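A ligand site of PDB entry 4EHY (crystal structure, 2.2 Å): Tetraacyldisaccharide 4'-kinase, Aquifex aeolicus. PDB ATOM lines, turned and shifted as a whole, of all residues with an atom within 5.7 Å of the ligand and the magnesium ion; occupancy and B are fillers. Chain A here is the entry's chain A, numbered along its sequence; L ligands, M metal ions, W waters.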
ATOM      1  N   GLY A  47      22.568 -16.150 -27.286  1.00  0.00           N
ATOM      2  CA  GLY A  47      22.186 -17.498 -26.923  1.00  0.00           C
ATOM      3  C   GLY A  47      22.967 -18.113 -25.777  1.00  0.00           C
ATOM      4  O   GLY A  47      22.987 -19.334 -25.608  1.00  0.00           O
ATOM      5  N   GLY A  48      23.622 -17.283 -24.973  1.00  0.00           N
ATOM      6  CA  GLY A  48      24.311 -17.780 -23.792  1.00  0.00           C
ATOM      7  C   GLY A  48      25.615 -18.495 -24.077  1.00  0.00           C
ATOM      8  O   GLY A  48      25.743 -19.252 -25.049  1.00  0.00           O
ATOM      9  N   SER A  49      26.571 -18.310 -23.187  1.00  0.00           N
ATOM     10  CA  SER A  49      27.934 -18.694 -23.455  1.00  0.00           C
ATOM     11  C   SER A  49      28.751 -18.743 -22.209  1.00  0.00           C
ATOM     12  O   SER A  49      29.978 -18.757 -22.272  1.00  0.00           O
ATOM     13  CB  SER A  49      28.541 -17.651 -24.369  1.00  0.00           C
ATOM     14  OG  SER A  49      28.044 -16.383 -23.963  1.00  0.00           O
ATOM     15  N   GLY A  50      28.096 -18.756 -21.049  1.00  0.00           N
ATOM     16  CA  GLY A  50      28.805 -18.843 -19.791  1.00  0.00           C
ATOM     17  C   GLY A  50      29.336 -17.506 -19.283  1.00  0.00           C
ATOM     18  O   GLY A  50      30.139 -17.472 -18.327  1.00  0.00           O
ATOM     19  N   LYS A  51      28.873 -16.418 -19.889  1.00  0.00           N
ATOM     20  CA  LYS A  51      29.356 -15.064 -19.529  1.00  0.00           C
ATOM     21  C   LYS A  51      29.082 -14.702 -18.086  1.00  0.00           C
ATOM     22  O   LYS A  51      29.989 -14.287 -17.359  1.00  0.00           O
ATOM     23  CB  LYS A  51      28.707 -13.980 -20.420  1.00  0.00           C
ATOM     24  CG  LYS A  51      29.064 -14.085 -21.886  1.00  0.00           C
ATOM     25  CD  LYS A  51      28.628 -12.823 -22.668  1.00  0.00           C
ATOM     26  CE  LYS A  51      27.121 -12.545 -22.532  1.00  0.00           C
ATOM     27  NZ  LYS A  51      26.245 -13.603 -23.116  1.00  0.00           N
ATOM     28  N   THR A  52      27.834 -14.869 -17.660  1.00  0.00           N
ATOM     29  CA  THR A  52      27.463 -14.491 -16.297  1.00  0.00           C
ATOM     30  C   THR A  52      28.242 -15.355 -15.326  1.00  0.00           C
ATOM     31  O   THR A  52      28.797 -14.853 -14.345  1.00  0.00           O
ATOM     32  CB  THR A  52      25.955 -14.722 -16.058  1.00  0.00           C
ATOM     33  OG1 THR A  52      25.207 -14.115 -17.117  1.00  0.00           O
ATOM     34  CG2 THR A  52      25.511 -14.135 -14.745  1.00  0.00           C
ATOM     35  N   SER A  53      28.314 -16.658 -15.597  1.00  0.00           N
ATOM     36  CA  SER A  53      29.053 -17.558 -14.706  1.00  0.00           C
ATOM     37  C   SER A  53      30.528 -17.177 -14.698  1.00  0.00           C
ATOM     38  O   SER A  53      31.166 -17.154 -13.646  1.00  0.00           O
ATOM     39  CB  SER A  53      28.877 -19.024 -15.135  1.00  0.00           C
ATOM     40  OG  SER A  53      27.514 -19.416 -15.001  1.00  0.00           O
ATOM     41  N   MET A  56      31.226 -14.154 -12.598  1.00  0.00           N
ATOM     42  CA  MET A  56      31.196 -14.488 -11.175  1.00  0.00           C
ATOM     43  C   MET A  56      32.446 -15.260 -10.765  1.00  0.00           C
ATOM     44  O   MET A  56      33.020 -15.037  -9.686  1.00  0.00           O
ATOM     45  CB  MET A  56      29.927 -15.280 -10.811  1.00  0.00           C
ATOM     46  CG  MET A  56      28.660 -14.487 -11.090  1.00  0.00           C
ATOM     47  SD  MET A  56      27.149 -15.308 -10.530  1.00  0.00           S
ATOM     48  CE  MET A  56      27.115 -16.735 -11.591  1.00  0.00           C
ATOM     49  N   GLU A 100      20.240 -10.972 -14.795  1.00  0.00           N
ATOM     50  CA  GLU A 100      21.670 -11.282 -14.665  1.00  0.00           C
ATOM     51  C   GLU A 100      22.400 -10.397 -13.660  1.00  0.00           C
ATOM     52  O   GLU A 100      23.107 -10.908 -12.789  1.00  0.00           O
ATOM     53  CB  GLU A 100      22.360 -11.321 -16.026  1.00  0.00           C
ATOM     54  CG  GLU A 100      21.888 -12.540 -16.838  1.00  0.00           C
ATOM     55  CD  GLU A 100      21.988 -12.325 -18.329  1.00  0.00           C
ATOM     56  OE1 GLU A 100      21.766 -13.291 -19.092  1.00  0.00           O
ATOM     57  OE2 GLU A 100      22.296 -11.180 -18.737  1.00  0.00           O
ATOM     58  N   LEU A 103      21.340 -11.465 -10.272  1.00  0.00           N
ATOM     59  CA  LEU A 103      21.903 -12.756  -9.871  1.00  0.00           C
ATOM     60  C   LEU A 103      23.339 -12.583  -9.416  1.00  0.00           C
ATOM     61  O   LEU A 103      23.733 -13.106  -8.364  1.00  0.00           O
ATOM     62  CB  LEU A 103      21.843 -13.763 -11.016  1.00  0.00           C
ATOM     63  CG  LEU A 103      22.419 -15.169 -10.706  1.00  0.00           C
ATOM     64  CD1 LEU A 103      21.493 -15.950  -9.754  1.00  0.00           C
ATOM     65  CD2 LEU A 103      22.646 -15.954 -11.982  1.00  0.00           C
ATOM     66  N   TYR A 187      31.546 -24.514 -21.901  1.00  0.00           N
ATOM     67  CA  TYR A 187      30.741 -25.735 -22.004  1.00  0.00           C
ATOM     68  C   TYR A 187      31.551 -26.982 -22.293  1.00  0.00           C
ATOM     69  O   TYR A 187      31.072 -27.889 -22.972  1.00  0.00           O
ATOM     70  CB  TYR A 187      29.643 -25.591 -23.068  1.00  0.00           C
ATOM     71  CG  TYR A 187      28.660 -24.478 -22.819  1.00  0.00           C
ATOM     72  CD1 TYR A 187      27.886 -23.987 -23.860  1.00  0.00           C
ATOM     73  CD2 TYR A 187      28.503 -23.906 -21.563  1.00  0.00           C
ATOM     74  CE1 TYR A 187      26.988 -22.970 -23.667  1.00  0.00           C
ATOM     75  CE2 TYR A 187      27.591 -22.863 -21.361  1.00  0.00           C
ATOM     76  CZ  TYR A 187      26.839 -22.412 -22.427  1.00  0.00           C
ATOM     77  OH  TYR A 187      25.931 -21.394 -22.275  1.00  0.00           O
ATOM     78  N   ARG A 206      31.934 -26.543 -16.115  1.00  0.00           N
ATOM     79  CA  ARG A 206      30.983 -26.323 -15.027  1.00  0.00           C
ATOM     80  C   ARG A 206      30.839 -27.633 -14.258  1.00  0.00           C
ATOM     81  O   ARG A 206      30.494 -28.674 -14.832  1.00  0.00           O
ATOM     82  CB  ARG A 206      29.639 -25.817 -15.563  1.00  0.00           C
ATOM     83  CG  ARG A 206      29.661 -24.354 -16.014  1.00  0.00           C
ATOM     84  CD  ARG A 206      28.352 -23.938 -16.691  1.00  0.00           C
ATOM     85  NE  ARG A 206      27.954 -24.909 -17.698  1.00  0.00           N
ATOM     86  CZ  ARG A 206      26.844 -24.844 -18.418  1.00  0.00           C
ATOM     87  NH1 ARG A 206      26.005 -23.836 -18.239  1.00  0.00           N
ATOM     88  NH2 ARG A 206      26.573 -25.802 -19.292  1.00  0.00           N
ATOM     89  N   PHE A 208      28.765 -29.548 -11.821  1.00  0.00           N
ATOM     90  CA  PHE A 208      27.429 -29.559 -11.243  1.00  0.00           C
ATOM     91  C   PHE A 208      27.418 -30.396  -9.982  1.00  0.00           C
ATOM     92  O   PHE A 208      27.329 -31.602 -10.028  1.00  0.00           O
ATOM     93  CB  PHE A 208      26.420 -30.083 -12.273  1.00  0.00           C
ATOM     94  CG  PHE A 208      26.352 -29.226 -13.496  1.00  0.00           C
ATOM     95  CD1 PHE A 208      27.092 -29.540 -14.623  1.00  0.00           C
ATOM     96  CD2 PHE A 208      25.588 -28.062 -13.487  1.00  0.00           C
ATOM     97  CE1 PHE A 208      27.041 -28.722 -15.736  1.00  0.00           C
ATOM     98  CE2 PHE A 208      25.532 -27.252 -14.597  1.00  0.00           C
ATOM     99  CZ  PHE A 208      26.261 -27.574 -15.729  1.00  0.00           C
ATOM    100  N   GLY A 234      14.596 -20.351 -18.415  1.00  0.00           N
ATOM    101  CA  GLY A 234      14.399 -19.255 -19.340  1.00  0.00           C
ATOM    102  C   GLY A 234      15.787 -18.662 -19.481  1.00  0.00           C
ATOM    103  O   GLY A 234      16.159 -17.746 -18.743  1.00  0.00           O
ATOM    104  N   LEU A 235      16.545 -19.203 -20.425  1.00  0.00           N
ATOM    105  CA  LEU A 235      17.961 -18.948 -20.580  1.00  0.00           C
ATOM    106  C   LEU A 235      18.235 -18.550 -22.033  1.00  0.00           C
ATOM    107  O   LEU A 235      17.356 -18.615 -22.891  1.00  0.00           O
ATOM    108  CB  LEU A 235      18.823 -20.174 -20.270  1.00  0.00           C
ATOM    109  CG  LEU A 235      18.477 -20.906 -18.969  1.00  0.00           C
ATOM    110  CD1 LEU A 235      19.260 -22.201 -18.869  1.00  0.00           C
ATOM    111  CD2 LEU A 235      18.760 -20.010 -17.790  1.00  0.00           C
ATOM    112  N   GLY A 236      19.478 -18.177 -22.303  1.00  0.00           N
ATOM    113  CA  GLY A 236      19.911 -17.981 -23.678  1.00  0.00           C
ATOM    114  C   GLY A 236      19.728 -19.246 -24.499  1.00  0.00           C
ATOM    115  O   GLY A 236      19.348 -19.186 -25.662  1.00  0.00           O
ATOM    116  N   ASP A 237      20.022 -20.391 -23.900  1.00  0.00           N
ATOM    117  CA  ASP A 237      19.817 -21.679 -24.576  1.00  0.00           C
ATOM    118  C   ASP A 237      19.366 -22.741 -23.584  1.00  0.00           C
ATOM    119  O   ASP A 237      20.177 -23.273 -22.830  1.00  0.00           O
ATOM    120  CB  ASP A 237      21.098 -22.114 -25.302  1.00  0.00           C
ATOM    121  CG  ASP A 237      20.951 -23.444 -26.039  1.00  0.00           C
ATOM    122  OD1 ASP A 237      19.809 -23.932 -26.205  1.00  0.00           O
ATOM    123  OD2 ASP A 237      21.986 -23.999 -26.460  1.00  0.00           O
ATOM    124  N   GLN A 240      21.053 -26.623 -23.471  1.00  0.00           N
ATOM    125  CA  GLN A 240      22.218 -27.137 -22.746  1.00  0.00           C
ATOM    126  C   GLN A 240      21.888 -27.498 -21.293  1.00  0.00           C
ATOM    127  O   GLN A 240      22.508 -28.380 -20.708  1.00  0.00           O
ATOM    128  CB  GLN A 240      23.416 -26.180 -22.826  1.00  0.00           C
ATOM    129  CG  GLN A 240      23.121 -24.751 -22.447  1.00  0.00           C
ATOM    130  CD  GLN A 240      23.175 -24.513 -20.954  1.00  0.00           C
ATOM    131  OE1 GLN A 240      23.868 -25.218 -20.216  1.00  0.00           O
ATOM    132  NE2 GLN A 240      22.442 -23.501 -20.498  1.00  0.00           N
ATOM    133  N   PHE A 241      20.901 -26.818 -20.725  1.00  0.00           N
ATOM    134  CA  PHE A 241      20.439 -27.150 -19.377  1.00  0.00           C
ATOM    135  C   PHE A 241      19.778 -28.518 -19.441  1.00  0.00           C
ATOM    136  O   PHE A 241      20.085 -29.414 -18.651  1.00  0.00           O
ATOM    137  CB  PHE A 241      19.445 -26.084 -18.882  1.00  0.00           C
ATOM    138  CG  PHE A 241      18.858 -26.378 -17.524  1.00  0.00           C
ATOM    139  CD1 PHE A 241      19.663 -26.823 -16.480  1.00  0.00           C
ATOM    140  CD2 PHE A 241      17.498 -26.226 -17.304  1.00  0.00           C
ATOM    141  CE1 PHE A 241      19.123 -27.080 -15.226  1.00  0.00           C
ATOM    142  CE2 PHE A 241      16.941 -26.484 -16.050  1.00  0.00           C
ATOM    143  CZ  PHE A 241      17.755 -26.900 -15.012  1.00  0.00           C
ATOM    144  N   VAL A 244      22.438 -31.164 -19.706  1.00  0.00           N
ATOM    145  CA  VAL A 244      23.138 -31.359 -18.441  1.00  0.00           C
ATOM    146  C   VAL A 244      22.318 -32.270 -17.533  1.00  0.00           C
ATOM    147  O   VAL A 244      22.860 -33.155 -16.873  1.00  0.00           O
ATOM    148  CB  VAL A 244      23.418 -30.016 -17.732  1.00  0.00           C
ATOM    149  CG1 VAL A 244      23.867 -30.253 -16.289  1.00  0.00           C
ATOM    150  CG2 VAL A 244      24.474 -29.211 -18.495  1.00  0.00           C
ATOM    151  N   ASP A 260      14.342 -16.423 -22.843  1.00  0.00           N
ATOM    152  CA  ASP A 260      15.408 -15.864 -22.018  1.00  0.00           C
ATOM    153  C   ASP A 260      14.842 -14.726 -21.182  1.00  0.00           C
ATOM    154  O   ASP A 260      14.044 -13.913 -21.673  1.00  0.00           O
ATOM    155  CB  ASP A 260      16.553 -15.373 -22.907  1.00  0.00           C
ATOM    156  CG  ASP A 260      17.824 -15.107 -22.129  1.00  0.00           C
ATOM    157  OD1 ASP A 260      18.830 -14.724 -22.758  1.00  0.00           O
ATOM    158  OD2 ASP A 260      17.811 -15.276 -20.886  1.00  0.00           O
ATOM    159  N   HIS A 261      15.214 -14.665 -19.908  1.00  0.00           N
ATOM    160  CA  HIS A 261      14.806 -13.558 -19.044  1.00  0.00           C
ATOM    161  C   HIS A 261      13.319 -13.592 -18.714  1.00  0.00           C
ATOM    162  O   HIS A 261      12.750 -12.603 -18.233  1.00  0.00           O
ATOM    163  CB  HIS A 261      15.166 -12.220 -19.715  1.00  0.00           C
ATOM    164  CG  HIS A 261      16.604 -12.122 -20.122  1.00  0.00           C
ATOM    165  ND1 HIS A 261      17.637 -12.117 -19.197  1.00  0.00           N
ATOM    166  CD2 HIS A 261      17.191 -12.027 -21.345  1.00  0.00           C
ATOM    167  CE1 HIS A 261      18.799 -12.005 -19.841  1.00  0.00           C
ATOM    168  NE2 HIS A 261      18.552 -11.956 -21.139  1.00  0.00           N
ATOM    169  N   THR A 277      15.205 -26.053 -11.687  1.00  0.00           N
ATOM    170  CA  THR A 277      15.515 -24.985 -12.621  1.00  0.00           C
ATOM    171  C   THR A 277      16.898 -24.413 -12.280  1.00  0.00           C
ATOM    172  O   THR A 277      17.615 -25.012 -11.475  1.00  0.00           O
ATOM    173  CB  THR A 277      14.433 -23.864 -12.559  1.00  0.00           C
ATOM    174  OG1 THR A 277      14.643 -22.927 -13.618  1.00  0.00           O
ATOM    175  CG2 THR A 277      14.428 -23.142 -11.201  1.00  0.00           C
ATOM    176  N   THR A 278      17.285 -23.288 -12.894  1.00  0.00           N
ATOM    177  CA  THR A 278      18.610 -22.691 -12.611  1.00  0.00           C
ATOM    178  C   THR A 278      18.604 -21.504 -11.653  1.00  0.00           C
ATOM    179  O   THR A 278      17.549 -20.946 -11.339  1.00  0.00           O
ATOM    180  CB  THR A 278      19.252 -22.230 -13.947  1.00  0.00           C
ATOM    181  OG1 THR A 278      18.681 -20.983 -14.342  1.00  0.00           O
ATOM    182  CG2 THR A 278      19.029 -23.246 -15.044  1.00  0.00           C
ATOM    183  N   PRO A 279      19.794 -21.103 -11.183  1.00  0.00           N
ATOM    184  CA  PRO A 279      19.805 -19.971 -10.260  1.00  0.00           C
ATOM    185  C   PRO A 279      19.226 -18.712 -10.924  1.00  0.00           C
ATOM    186  O   PRO A 279      18.573 -17.901 -10.278  1.00  0.00           O
ATOM    187  CB  PRO A 279      21.292 -19.794  -9.946  1.00  0.00           C
ATOM    188  CG  PRO A 279      21.838 -21.212 -10.071  1.00  0.00           C
ATOM    189  CD  PRO A 279      21.100 -21.785 -11.254  1.00  0.00           C
ATOM    190  N   LYS A 280      19.437 -18.588 -12.224  1.00  0.00           N
ATOM    191  CA  LYS A 280      18.973 -17.423 -12.974  1.00  0.00           C
ATOM    192  C   LYS A 280      17.462 -17.334 -12.917  1.00  0.00           C
ATOM    193  O   LYS A 280      16.890 -16.246 -12.758  1.00  0.00           O
ATOM    194  CB  LYS A 280      19.488 -17.487 -14.424  1.00  0.00           C
ATOM    195  CG  LYS A 280      18.981 -16.362 -15.325  1.00  0.00           C
ATOM    196  CD  LYS A 280      19.619 -16.454 -16.711  1.00  0.00           C
ATOM    197  CE  LYS A 280      18.959 -15.486 -17.702  1.00  0.00           C
ATOM    198  NZ  LYS A 280      19.750 -15.371 -18.976  1.00  0.00           N
ATOM    199  N   LEU A 294      19.596 -26.336  -9.828  1.00  0.00           N
ATOM    200  CA  LEU A 294      20.880 -27.002  -9.980  1.00  0.00           C
ATOM    201  C   LEU A 294      21.961 -25.938  -9.949  1.00  0.00           C
ATOM    202  O   LEU A 294      21.874 -24.927 -10.670  1.00  0.00           O
ATOM    203  CB  LEU A 294      20.939 -27.756 -11.301  1.00  0.00           C
ATOM    204  CG  LEU A 294      22.216 -28.559 -11.591  1.00  0.00           C
ATOM    205  CD1 LEU A 294      22.362 -29.704 -10.597  1.00  0.00           C
ATOM    206  CD2 LEU A 294      22.185 -29.103 -13.012  1.00  0.00           C
ATOM    207  N   ASN A 295      22.968 -26.137  -9.112  1.00  0.00           N
ATOM    208  CA  ASN A 295      24.041 -25.164  -8.979  1.00  0.00           C
ATOM    209  C   ASN A 295      25.347 -25.862  -9.337  1.00  0.00           C
ATOM    210  O   ASN A 295      25.393 -27.077  -9.400  1.00  0.00           O
ATOM    211  CB  ASN A 295      24.064 -24.599  -7.554  1.00  0.00           C
ATOM    212  CG  ASN A 295      24.791 -23.269  -7.474  1.00  0.00           C
ATOM    213  OD1 ASN A 295      25.002 -22.582  -8.482  1.00  0.00           O
ATOM    214  ND2 ASN A 295      25.179 -22.884  -6.262  1.00  0.00           N
ATOM    215  N   PHE A 296      26.389 -25.094  -9.612  1.00  0.00           N
ATOM    216  CA  PHE A 296      27.658 -25.647 -10.079  1.00  0.00           C
ATOM    217  C   PHE A 296      28.825 -24.727  -9.696  1.00  0.00           C
ATOM    218  O   PHE A 296      28.612 -23.559  -9.367  1.00  0.00           O
ATOM    219  CB  PHE A 296      27.627 -25.797 -11.599  1.00  0.00           C
ATOM    220  CG  PHE A 296      27.302 -24.515 -12.311  1.00  0.00           C
ATOM    221  CD1 PHE A 296      28.319 -23.658 -12.738  1.00  0.00           C
ATOM    222  CD2 PHE A 296      25.985 -24.135 -12.516  1.00  0.00           C
ATOM    223  CE1 PHE A 296      28.022 -22.455 -13.383  1.00  0.00           C
ATOM    224  CE2 PHE A 296      25.670 -22.927 -13.150  1.00  0.00           C
ATOM    225  CZ  PHE A 296      26.693 -22.076 -13.580  1.00  0.00           C
HETATM  226  P1  LIG L   1      24.876 -15.977 -20.346  1.00  0.00           P
HETATM  227  O1  LIG L   1      23.813 -14.910 -20.511  1.00  0.00           O
HETATM  228  O2  LIG L   1      25.846 -16.058 -21.496  1.00  0.00           O
HETATM  229  O3  LIG L   1      25.579 -15.883 -19.015  1.00  0.00           O
HETATM  230  P2  LIG L   1      22.716 -17.911 -19.790  1.00  0.00           P
HETATM  231  O4  LIG L   1      22.933 -19.397 -19.818  1.00  0.00           O
HETATM  232  O5  LIG L   1      21.488 -17.306 -20.415  1.00  0.00           O
HETATM  233  O6  LIG L   1      24.104 -17.381 -20.456  1.00  0.00           O
HETATM  234  O7  LIG L   1      22.719 -17.430 -18.267  1.00  0.00           O
HETATM  235  C1  LIG L   1      23.738 -17.872 -17.375  1.00  0.00           C
HETATM  236  C2  LIG L   1      23.054 -18.228 -16.072  1.00  0.00           C
HETATM  237  O8  LIG L   1      21.956 -19.142 -16.310  1.00  0.00           O
HETATM  238  C3  LIG L   1      24.028 -18.965 -15.183  1.00  0.00           C
HETATM  239  O9  LIG L   1      24.703 -18.050 -14.334  1.00  0.00           O
HETATM  240  C4  LIG L   1      23.153 -19.932 -14.418  1.00  0.00           C
HETATM  241  O10 LIG L   1      22.579 -19.233 -13.309  1.00  0.00           O
HETATM  242  C5  LIG L   1      22.024 -20.228 -15.384  1.00  0.00           C
HETATM  243  N1  LIG L   1      22.352 -21.467 -16.146  1.00  0.00           N
HETATM  244  C6  LIG L   1      22.569 -21.540 -17.472  1.00  0.00           C
HETATM  245  N2  LIG L   1      22.823 -22.816 -17.862  1.00  0.00           N
HETATM  246  C7  LIG L   1      22.766 -23.593 -16.762  1.00  0.00           C
HETATM  247  C8  LIG L   1      22.934 -25.040 -16.472  1.00  0.00           C
HETATM  248  N3  LIG L   1      23.231 -25.945 -17.457  1.00  0.00           N
HETATM  249  N4  LIG L   1      22.780 -25.414 -15.182  1.00  0.00           N
HETATM  250  C9  LIG L   1      22.485 -24.537 -14.198  1.00  0.00           C
HETATM  251  N5  LIG L   1      22.325 -23.221 -14.396  1.00  0.00           N
HETATM  252  C10 LIG L   1      22.442 -22.696 -15.640  1.00  0.00           C
HETATM  253 MG    MG M   1      22.652 -13.298 -21.133  1.00  0.00          MG
HETATM  254  O   HOH W   1      21.461 -11.723 -21.794  1.00  0.00           O
HETATM  255  O   HOH W   2      21.879 -20.772 -21.969  1.00  0.00           O
HETATM  256  O   HOH W   3      26.872 -17.919 -17.685  1.00  0.00           O
HETATM  257  O   HOH W   4      21.230 -14.734 -21.773  1.00  0.00           O
HETATM  258  O   HOH W   5      24.155 -11.998 -20.640  1.00  0.00           O
HETATM  259  O   HOH W   6      25.459 -19.889 -19.915  1.00  0.00           O
HETATM  260  O   HOH W   7      23.561 -13.217 -23.034  1.00  0.00           O
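CA of Gly 48 touches O2 of the ligand, 3.3 Å away. N of Gly 50 touches O2 of the ligand, at 3.5 Å. Met 56 touches the ligand (CE to O9, 3.9 Å). CD2 of Leu 103 touches O10 of the ligand, at 3.5 Å. Phe 208 touches the ligand. CD2 of Leu 235 touches O8 of the ligand, at 3.6 Å. Phe 241 touches the ligand (CA to N3, 3.6 Å). Val 244 touches the ligand (CG2 to N3, 3.6 Å). Thr 278 touches the ligand (CB to N5, 3.3 Å). Pro 279 touches the ligand (CD to O10, 3.6 Å). Leu 294 touches the ligand. CE2 of Phe 296 touches N5 of the ligand (3.6 Å).
The magnesium ion is bound by water W5, O1 of the ligand, water W1, water W7, water W4 and OE1 of Glu 100.
Of the 29 residues printed, 1 comes within 4 Å of the magnesium ion.
The backbone NH (N) of Ser 49 sits at hydrogen-bond distance from an oxygen (O2) of the ligand, 2.9 Å away. NZ of Lys 280 lies within salt-bridge range of O5 of the ligand. N2 of the ligand lies within hydrogen-bond range of NE2 of Gln 240. OG of Ser 49 is in hydrogen-bond range of O2 of the ligand, at 3.3 Å. The guanidinium group (NH1) of Arg 206 sits at hydrogen-bond distance from a nitrogen (N2) of the ligand (3.4 Å). O5 of the ligand sits at hydrogen-bond distance from N of Gly 236 (2.9 Å). An oxygen (O2) of the ligand is in salt-bridge range of the side-chain amino group (NZ) of Lys 51 (3.0 Å). OG1 of Thr 52 is in hydrogen-bond range of O3 of the ligand, at 2.6 Å. The backbone NH of Lys 51 is in hydrogen-bond range of an oxygen (O2) of the ligand (3.4 Å). OG of Ser 53 is in hydrogen-bond range of O9 of the ligand. N of Lys 280 is in hydrogen-bond range of O10 of the ligand. N of Thr 52 is in hydrogen-bond range of O3 of the ligand (2.8 Å).
The side-chain amino group (NZ) of Lys 280 is in salt-bridge range of the side-chain carboxylate (OD2) of Asp 260, at 2.7 Å. N of Ser 49 sits at hydrogen-bond distance from OH of Tyr 187, 3.3 Å away. OE1 of Gln 240 lies within hydrogen-bond range of NH2 of Arg 206 (2.9 Å). OG of Ser 49 sits close to NZ of Lys 51, at 3.4 Å. The side-chain amino group (NZ) of Lys 280 lies close to the side-chain carboxylate (OE1) of Glu 100 (2.9 Å). O of Thr 277 lies within hydrogen-bond range of N of Leu 294 (2.9 Å). The backbone NH (N) of Lys 280 lies close to the side-chain hydroxyl (OG1) of Thr 278. The side-chain amide nitrogen (NE2) of Gln 240 is in hydrogen-bond range of the backbone carbonyl oxygen (O) of Asp 237 (3.3 Å).
Water W1 lies within hydrogen-bond range of a ring nitrogen (NE2) of His 261 and the side-chain carboxylate (OE2) of Glu 100. Water W4 lies within hydrogen-bond range of OD1 of Asp 260 (2.6 Å), O5 of the ligand (2.9 Å) and NZ of Lys 280 (3.2 Å). Water W6 lies within hydrogen-bond range of O4 of the ligand, OH of Tyr 187 and N of Gly 50. Water W2 lies within hydrogen-bond range of the backbone NH of Asp 237, an oxygen (O4) of the ligand and the side-chain amide nitrogen of Gln 240.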
